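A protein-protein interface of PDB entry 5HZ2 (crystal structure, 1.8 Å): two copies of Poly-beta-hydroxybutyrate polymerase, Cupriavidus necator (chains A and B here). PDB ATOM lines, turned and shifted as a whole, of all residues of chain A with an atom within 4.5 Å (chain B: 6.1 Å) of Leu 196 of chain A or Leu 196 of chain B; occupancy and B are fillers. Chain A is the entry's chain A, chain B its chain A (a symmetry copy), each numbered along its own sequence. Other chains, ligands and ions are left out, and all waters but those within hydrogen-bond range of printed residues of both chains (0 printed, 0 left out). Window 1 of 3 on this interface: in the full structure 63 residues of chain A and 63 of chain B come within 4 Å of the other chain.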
ATOM      1  N   ILE A 156       7.721 -16.914   9.402  1.00  0.00           N
ATOM      2  CA  ILE A 156       8.203 -15.902   8.473  1.00  0.00           C
ATOM      3  C   ILE A 156       9.610 -15.383   8.840  1.00  0.00           C
ATOM      4  O   ILE A 156      10.377 -14.979   7.999  1.00  0.00           O
ATOM      5  CB  ILE A 156       7.111 -14.916   7.979  1.00  0.00           C
ATOM      6  CG1 ILE A 156       7.321 -13.503   8.448  1.00  0.00           C
ATOM      7  CG2 ILE A 156       5.722 -15.406   8.319  1.00  0.00           C
ATOM      8  CD1 ILE A 156       6.193 -12.612   7.991  1.00  0.00           C
ATOM      9  N   SER A 194      -1.528 -19.049  -0.739  1.00  0.00           N
ATOM     10  CA  SER A 194      -0.271 -18.409  -1.033  1.00  0.00           C
ATOM     11  C   SER A 194      -0.122 -17.048  -0.351  1.00  0.00           C
ATOM     12  O   SER A 194       0.582 -16.196  -0.830  1.00  0.00           O
ATOM     13  CB  SER A 194      -0.036 -18.359  -2.533  1.00  0.00           C
ATOM     14  OG  SER A 194      -0.012 -19.671  -3.046  1.00  0.00           O
ATOM     15  N   PHE A 195      -0.815 -16.850   0.761  1.00  0.00           N
ATOM     16  CA  PHE A 195      -0.714 -15.578   1.444  1.00  0.00           C
ATOM     17  C   PHE A 195       0.735 -15.319   1.869  1.00  0.00           C
ATOM     18  O   PHE A 195       1.214 -14.214   1.800  1.00  0.00           O
ATOM     19  CB  PHE A 195      -1.659 -15.457   2.633  1.00  0.00           C
ATOM     20  CG  PHE A 195      -1.562 -14.133   3.314  1.00  0.00           C
ATOM     21  CD1 PHE A 195      -1.918 -12.980   2.659  1.00  0.00           C
ATOM     22  CD2 PHE A 195      -1.050 -14.033   4.571  1.00  0.00           C
ATOM     23  CE1 PHE A 195      -1.798 -11.754   3.267  1.00  0.00           C
ATOM     24  CE2 PHE A 195      -0.921 -12.812   5.185  1.00  0.00           C
ATOM     25  CZ  PHE A 195      -1.303 -11.671   4.535  1.00  0.00           C
ATOM     26  N   LEU A 196       1.437 -16.345   2.305  1.00  0.00           N
ATOM     27  CA  LEU A 196       2.835 -16.157   2.710  1.00  0.00           C
ATOM     28  C   LEU A 196       3.762 -16.635   1.610  1.00  0.00           C
ATOM     29  O   LEU A 196       4.877 -17.003   1.848  1.00  0.00           O
ATOM     30  CB  LEU A 196       3.136 -16.897   3.993  1.00  0.00           C
ATOM     31  CG  LEU A 196       3.221 -16.080   5.270  1.00  0.00           C
ATOM     32  CD1 LEU A 196       2.389 -14.815   5.274  1.00  0.00           C
ATOM     33  CD2 LEU A 196       2.985 -16.971   6.469  1.00  0.00           C
ATOM     34  N   ARG A 197       3.243 -16.672   0.403  1.00  0.00           N
ATOM     35  CA  ARG A 197       3.965 -17.180  -0.735  1.00  0.00           C
ATOM     36  C   ARG A 197       3.875 -16.245  -1.909  1.00  0.00           C
ATOM     37  O   ARG A 197       3.177 -15.262  -1.865  1.00  0.00           O
ATOM     38  CB  ARG A 197       3.410 -18.542  -1.111  1.00  0.00           C
ATOM     39  CG  ARG A 197       3.611 -19.595  -0.041  1.00  0.00           C
ATOM     40  CD  ARG A 197       5.075 -19.948   0.058  1.00  0.00           C
ATOM     41  NE  ARG A 197       5.333 -21.108   0.891  1.00  0.00           N
ATOM     42  CZ  ARG A 197       6.524 -21.407   1.383  1.00  0.00           C
ATOM     43  NH1 ARG A 197       7.559 -20.628   1.125  1.00  0.00           N
ATOM     44  NH2 ARG A 197       6.688 -22.484   2.129  1.00  0.00           N
ATOM     45  N   PRO A 198       4.618 -16.529  -2.954  1.00  0.00           N
ATOM     46  CA  PRO A 198       4.488 -15.623  -4.100  1.00  0.00           C
ATOM     47  C   PRO A 198       3.086 -15.509  -4.627  1.00  0.00           C
ATOM     48  O   PRO A 198       2.277 -16.469  -4.524  1.00  0.00           O
ATOM     49  CB  PRO A 198       5.370 -16.290  -5.179  1.00  0.00           C
ATOM     50  CG  PRO A 198       6.366 -17.073  -4.370  1.00  0.00           C
ATOM     51  CD  PRO A 198       5.548 -17.626  -3.258  1.00  0.00           C
ATOM     52  N   TYR A 244       2.130 -11.310  12.304  1.00  0.00           N
ATOM     53  CA  TYR A 244       3.167 -12.211  11.890  1.00  0.00           C
ATOM     54  C   TYR A 244       4.572 -11.824  12.319  1.00  0.00           C
ATOM     55  O   TYR A 244       5.304 -12.670  12.771  1.00  0.00           O
ATOM     56  CB  TYR A 244       3.140 -12.440  10.345  1.00  0.00           C
ATOM     57  CG  TYR A 244       2.002 -13.293   9.904  1.00  0.00           C
ATOM     58  CD1 TYR A 244       2.140 -14.681   9.901  1.00  0.00           C
ATOM     59  CD2 TYR A 244       0.787 -12.765   9.439  1.00  0.00           C
ATOM     60  CE1 TYR A 244       1.141 -15.502   9.453  1.00  0.00           C
ATOM     61  CE2 TYR A 244      -0.251 -13.619   9.013  1.00  0.00           C
ATOM     62  CZ  TYR A 244      -0.051 -14.979   9.024  1.00  0.00           C
ATOM     63  OH  TYR A 244      -1.002 -15.905   8.647  1.00  0.00           O
ATOM     64  N   THR B 154      11.451 -29.235   0.434  1.00  0.00           N
ATOM     65  CA  THR B 154      11.667 -27.827   0.471  1.00  0.00           C
ATOM     66  C   THR B 154      10.366 -27.144   0.910  1.00  0.00           C
ATOM     67  O   THR B 154      10.344 -25.955   1.157  1.00  0.00           O
ATOM     68  CB  THR B 154      12.182 -27.299  -0.872  1.00  0.00           C
ATOM     69  OG1 THR B 154      11.476 -27.923  -1.970  1.00  0.00           O
ATOM     70  CG2 THR B 154      13.679 -27.604  -0.992  1.00  0.00           C
ATOM     71  N   ILE B 156       7.232 -26.454  -0.384  1.00  0.00           N
ATOM     72  CA  ILE B 156       6.223 -25.718  -1.132  1.00  0.00           C
ATOM     73  C   ILE B 156       4.893 -26.494  -1.252  1.00  0.00           C
ATOM     74  O   ILE B 156       3.832 -25.924  -1.346  1.00  0.00           O
ATOM     75  CB  ILE B 156       6.778 -24.925  -2.345  1.00  0.00           C
ATOM     76  CG1 ILE B 156       6.298 -25.444  -3.672  1.00  0.00           C
ATOM     77  CG2 ILE B 156       8.285 -24.830  -2.306  1.00  0.00           C
ATOM     78  CD1 ILE B 156       6.924 -24.676  -4.808  1.00  0.00           C
ATOM     79  N   ASN B 191      14.351 -12.214  -5.492  1.00  0.00           N
ATOM     80  CA  ASN B 191      15.398 -12.032  -4.526  1.00  0.00           C
ATOM     81  C   ASN B 191      15.580 -13.365  -3.824  1.00  0.00           C
ATOM     82  O   ASN B 191      14.714 -14.219  -3.857  1.00  0.00           O
ATOM     83  CB  ASN B 191      15.137 -10.895  -3.569  1.00  0.00           C
ATOM     84  CG  ASN B 191      13.879 -11.087  -2.779  1.00  0.00           C
ATOM     85  OD1 ASN B 191      13.071 -10.194  -2.696  1.00  0.00           O
ATOM     86  ND2 ASN B 191      13.716 -12.243  -2.192  1.00  0.00           N
ATOM     87  N   THR B 192      16.740 -13.554  -3.233  1.00  0.00           N
ATOM     88  CA  THR B 192      17.038 -14.797  -2.572  1.00  0.00           C
ATOM     89  C   THR B 192      16.238 -15.132  -1.308  1.00  0.00           C
ATOM     90  O   THR B 192      15.699 -16.209  -1.184  1.00  0.00           O
ATOM     91  CB  THR B 192      18.541 -14.824  -2.217  1.00  0.00           C
ATOM     92  OG1 THR B 192      19.320 -14.699  -3.408  1.00  0.00           O
ATOM     93  CG2 THR B 192      18.910 -16.094  -1.502  1.00  0.00           C
ATOM     94  N   PHE B 193      16.153 -14.189  -0.395  1.00  0.00           N
ATOM     95  CA  PHE B 193      15.474 -14.453   0.859  1.00  0.00           C
ATOM     96  C   PHE B 193      13.982 -14.680   0.784  1.00  0.00           C
ATOM     97  O   PHE B 193      13.418 -15.435   1.563  1.00  0.00           O
ATOM     98  CB  PHE B 193      15.939 -13.540   1.983  1.00  0.00           C
ATOM     99  CG  PHE B 193      17.275 -13.936   2.531  1.00  0.00           C
ATOM    100  CD1 PHE B 193      18.428 -13.634   1.843  1.00  0.00           C
ATOM    101  CD2 PHE B 193      17.377 -14.653   3.699  1.00  0.00           C
ATOM    102  CE1 PHE B 193      19.658 -14.014   2.323  1.00  0.00           C
ATOM    103  CE2 PHE B 193      18.604 -15.031   4.189  1.00  0.00           C
ATOM    104  CZ  PHE B 193      19.748 -14.710   3.500  1.00  0.00           C
ATOM    105  N   SER B 194      13.363 -13.991  -0.154  1.00  0.00           N
ATOM    106  CA  SER B 194      11.944 -14.092  -0.378  1.00  0.00           C
ATOM    107  C   SER B 194      11.596 -14.796  -1.691  1.00  0.00           C
ATOM    108  O   SER B 194      10.562 -14.555  -2.260  1.00  0.00           O
ATOM    109  CB  SER B 194      11.283 -12.733  -0.231  1.00  0.00           C
ATOM    110  OG  SER B 194      11.507 -12.243   1.071  1.00  0.00           O
ATOM    111  N   PHE B 195      12.487 -15.650  -2.173  1.00  0.00           N
ATOM    112  CA  PHE B 195      12.210 -16.340  -3.415  1.00  0.00           C
ATOM    113  C   PHE B 195      10.937 -17.182  -3.281  1.00  0.00           C
ATOM    114  O   PHE B 195      10.150 -17.266  -4.191  1.00  0.00           O
ATOM    115  CB  PHE B 195      13.376 -17.191  -3.903  1.00  0.00           C
ATOM    116  CG  PHE B 195      13.086 -17.878  -5.196  1.00  0.00           C
ATOM    117  CD1 PHE B 195      12.875 -17.153  -6.343  1.00  0.00           C
ATOM    118  CD2 PHE B 195      12.952 -19.231  -5.249  1.00  0.00           C
ATOM    119  CE1 PHE B 195      12.573 -17.777  -7.529  1.00  0.00           C
ATOM    120  CE2 PHE B 195      12.646 -19.863  -6.430  1.00  0.00           C
ATOM    121  CZ  PHE B 195      12.463 -19.136  -7.572  1.00  0.00           C
ATOM    122  N   LEU B 196      10.732 -17.802  -2.137  1.00  0.00           N
ATOM    123  CA  LEU B 196       9.521 -18.608  -1.947  1.00  0.00           C
ATOM    124  C   LEU B 196       8.505 -17.835  -1.132  1.00  0.00           C
ATOM    125  O   LEU B 196       7.670 -18.394  -0.479  1.00  0.00           O
ATOM    126  CB  LEU B 196       9.839 -19.918  -1.263  1.00  0.00           C
ATOM    127  CG  LEU B 196       9.884 -21.167  -2.126  1.00  0.00           C
ATOM    128  CD1 LEU B 196      10.263 -20.929  -3.573  1.00  0.00           C
ATOM    129  CD2 LEU B 196      10.711 -22.234  -1.445  1.00  0.00           C
ATOM    130  N   ARG B 197       8.640 -16.527  -1.144  1.00  0.00           N
ATOM    131  CA  ARG B 197       7.808 -15.656  -0.355  1.00  0.00           C
ATOM    132  C   ARG B 197       7.272 -14.514  -1.174  1.00  0.00           C
ATOM    133  O   ARG B 197       7.623 -14.352  -2.317  1.00  0.00           O
ATOM    134  CB  ARG B 197       8.613 -15.122   0.816  1.00  0.00           C
ATOM    135  CG  ARG B 197       9.054 -16.196   1.787  1.00  0.00           C
ATOM    136  CD  ARG B 197       7.858 -16.728   2.538  1.00  0.00           C
ATOM    137  NE  ARG B 197       8.210 -17.593   3.648  1.00  0.00           N
ATOM    138  CZ  ARG B 197       7.359 -18.418   4.235  1.00  0.00           C
ATOM    139  NH1 ARG B 197       6.110 -18.486   3.811  1.00  0.00           N
ATOM    140  NH2 ARG B 197       7.748 -19.171   5.247  1.00  0.00           N
ATOM    141  N   PRO B 198       6.380 -13.738  -0.601  1.00  0.00           N
ATOM    142  CA  PRO B 198       5.896 -12.612  -1.405  1.00  0.00           C
ATOM    143  C   PRO B 198       6.985 -11.689  -1.874  1.00  0.00           C
ATOM    144  O   PRO B 198       8.039 -11.539  -1.199  1.00  0.00           O
ATOM    145  CB  PRO B 198       4.983 -11.843  -0.424  1.00  0.00           C
ATOM    146  CG  PRO B 198       4.546 -12.909   0.541  1.00  0.00           C
ATOM    147  CD  PRO B 198       5.776 -13.721   0.739  1.00  0.00           C
ATOM    148  N   TRP B 203       5.191  -6.097   1.444  1.00  0.00           N
ATOM    149  CA  TRP B 203       6.080  -7.053   2.048  1.00  0.00           C
ATOM    150  C   TRP B 203       7.520  -6.564   2.099  1.00  0.00           C
ATOM    151  O   TRP B 203       8.169  -6.679   3.163  1.00  0.00           O
ATOM    152  CB  TRP B 203       6.009  -8.408   1.269  1.00  0.00           C
ATOM    153  CG  TRP B 203       7.071  -9.438   1.693  1.00  0.00           C
ATOM    154  CD1 TRP B 203       8.386  -9.540   1.242  1.00  0.00           C
ATOM    155  CD2 TRP B 203       6.913 -10.495   2.623  1.00  0.00           C
ATOM    156  NE1 TRP B 203       9.013 -10.579   1.831  1.00  0.00           N
ATOM    157  CE2 TRP B 203       8.143 -11.186   2.683  1.00  0.00           C
ATOM    158  CE3 TRP B 203       5.843 -10.958   3.397  1.00  0.00           C
ATOM    159  CZ2 TRP B 203       8.320 -12.301   3.481  1.00  0.00           C
ATOM    160  CZ3 TRP B 203       6.050 -12.110   4.191  1.00  0.00           C
ATOM    161  CH2 TRP B 203       7.260 -12.686   4.268  1.00  0.00           C
ATOM    162  N   LEU B 240      10.569 -23.544 -11.240  1.00  0.00           N
ATOM    163  CA  LEU B 240       9.593 -23.883 -10.233  1.00  0.00           C
ATOM    164  C   LEU B 240       8.941 -25.234 -10.479  1.00  0.00           C
ATOM    165  O   LEU B 240       8.804 -26.021  -9.581  1.00  0.00           O
ATOM    166  CB  LEU B 240       8.523 -22.805 -10.196  1.00  0.00           C
ATOM    167  CG  LEU B 240       7.407 -22.905  -9.187  1.00  0.00           C
ATOM    168  CD1 LEU B 240       7.983 -22.942  -7.786  1.00  0.00           C
ATOM    169  CD2 LEU B 240       6.471 -21.725  -9.349  1.00  0.00           C
ATOM    170  N   TYR B 244      11.470 -27.578  -7.584  1.00  0.00           N
ATOM    171  CA  TYR B 244      10.679 -27.489  -6.391  1.00  0.00           C
ATOM    172  C   TYR B 244       9.408 -28.322  -6.392  1.00  0.00           C
ATOM    173  O   TYR B 244       9.127 -28.968  -5.412  1.00  0.00           O
ATOM    174  CB  TYR B 244      10.327 -26.006  -6.051  1.00  0.00           C
ATOM    175  CG  TYR B 244      11.490 -25.239  -5.527  1.00  0.00           C
ATOM    176  CD1 TYR B 244      11.781 -25.269  -4.163  1.00  0.00           C
ATOM    177  CD2 TYR B 244      12.304 -24.434  -6.341  1.00  0.00           C
ATOM    178  CE1 TYR B 244      12.807 -24.537  -3.630  1.00  0.00           C
ATOM    179  CE2 TYR B 244      13.380 -23.710  -5.790  1.00  0.00           C
ATOM    180  CZ  TYR B 244      13.610 -23.773  -4.436  1.00  0.00           C
ATOM    181  OH  TYR B 244      14.644 -23.122  -3.794  1.00  0.00           O
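The guanidinium group (NH1) of Arg 197 of chain B sits at hydrogen-bond distance from the backbone carbonyl oxygen (O) of Leu 196 of chain A (2.8 Å).
The backbone carbonyl oxygen of Leu 196 of chain B sits at hydrogen-bond distance from the guanidinium group of Arg 197 of chain A (2.8 Å).
Of the 7 printed residues of chain A, 5 touch a printed residue of chain B.
Hydrophobic or aromatic side chains of chain A that line the printed part of chain B: Ile 156, Leu 196 and Pro 198.
Of the 13 printed residues of chain B, 5 touch a printed residue of chain A.
Printed residues of chain B that touch a printed residue of chain A: Phe 195, Leu 196, Arg 197, Pro 198 and Trp 203.
Along chain B the printed residues that touch a printed residue of chain A span positions 195 to 203.
O of Pro 198 of chain B lies close to NE1 of Trp 203 of chain B.
The side-chain hydroxyl (OG) of Ser 194 of chain B lies within hydrogen-bond range of the indole nitrogen (NE1) of Trp 203 of chain B, 3.1 Å away.
Among the printed residues, merely in contact across the chains: Leu 196 of chain A with Pro 198 of chain B (3.6 Å), Pro 198 of chain A with Leu 196 of chain B (3.6 Å), Pro 198 of chain A with Arg 197 of chain B (3.6 Å), Arg 197 of chain A with Pro 198 of chain B (3.6 Å), Arg 197 of chain A with Arg 197 of chain B (3.7 Å), Pro 198 of chain A with Phe 195 of chain B (3.8 Å), Phe 195 of chain A with Pro 198 of chain B (3.8 Å), Ile 156 of chain A with Trp 203 of chain B (3.8 Å) and Leu 196 of chain A with Leu 196 of chain B (3.9 Å).
Phe 195 of chain A touches Pro 198 of chain B, and with the chains exchanged Pro 198 of chain A touches Phe 195 of chain B.
Leu 196 of chain B touches its own counterpart, Leu 196 of chain A.
Leu 196 of chain A touches Arg 197 of chain B, and with the chains exchanged Arg 197 of chain A touches Leu 196 of chain B.
Leu 196 of chain A touches Pro 198 of chain B, and with the chains exchanged Pro 198 of chain A touches Leu 196 of chain B.
7 positions are printed for both chains.
Of chain B, only Leu 196 (3.9 Å), Arg 197 (2.8 Å) and Pro 198 (3.6 Å) come within 4 Å of Leu 196 of chain A.
Printed residues of chain A within 4 Å of Leu 196 of chain B: Leu 196, Arg 197 and Pro 198.
Printed residues of chain A within 4 Å of Pro 198 of chain B: Phe 195 (3.8 Å), Leu 196 (3.6 Å) and Arg 197 (3.6 Å).
Of the printed residues of chain A, Arg 197 of chain B touches Leu 196 (2.8 Å), Arg 197 (3.7 Å) and Pro 198 (3.6 Å).
Of the printed residues of chain B, Phe 195 of chain A touches Pro 198 (3.8 Å).
Of the printed residues of chain B, Pro 198 of chain A touches Phe 195, Leu 196 and Arg 197.
Printed residues of chain B within 4 Å of Arg 197 of chain A: Leu 196, Arg 197 and Pro 198.
Phe 193 of chain B touches none of the printed residues of chain A.
The nearest residue of chain B that does not touch Leu 196 of chain A is Trp 203 of chain B (4.7 Å).
The nearest printed residue of chain A that does not touch Leu 196 of chain B is Ser 194 of chain A (7.4 Å).
The nearest printed residue of chain B that does not touch Pro 198 of chain A is Pro 198 of chain B (4.1 Å).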
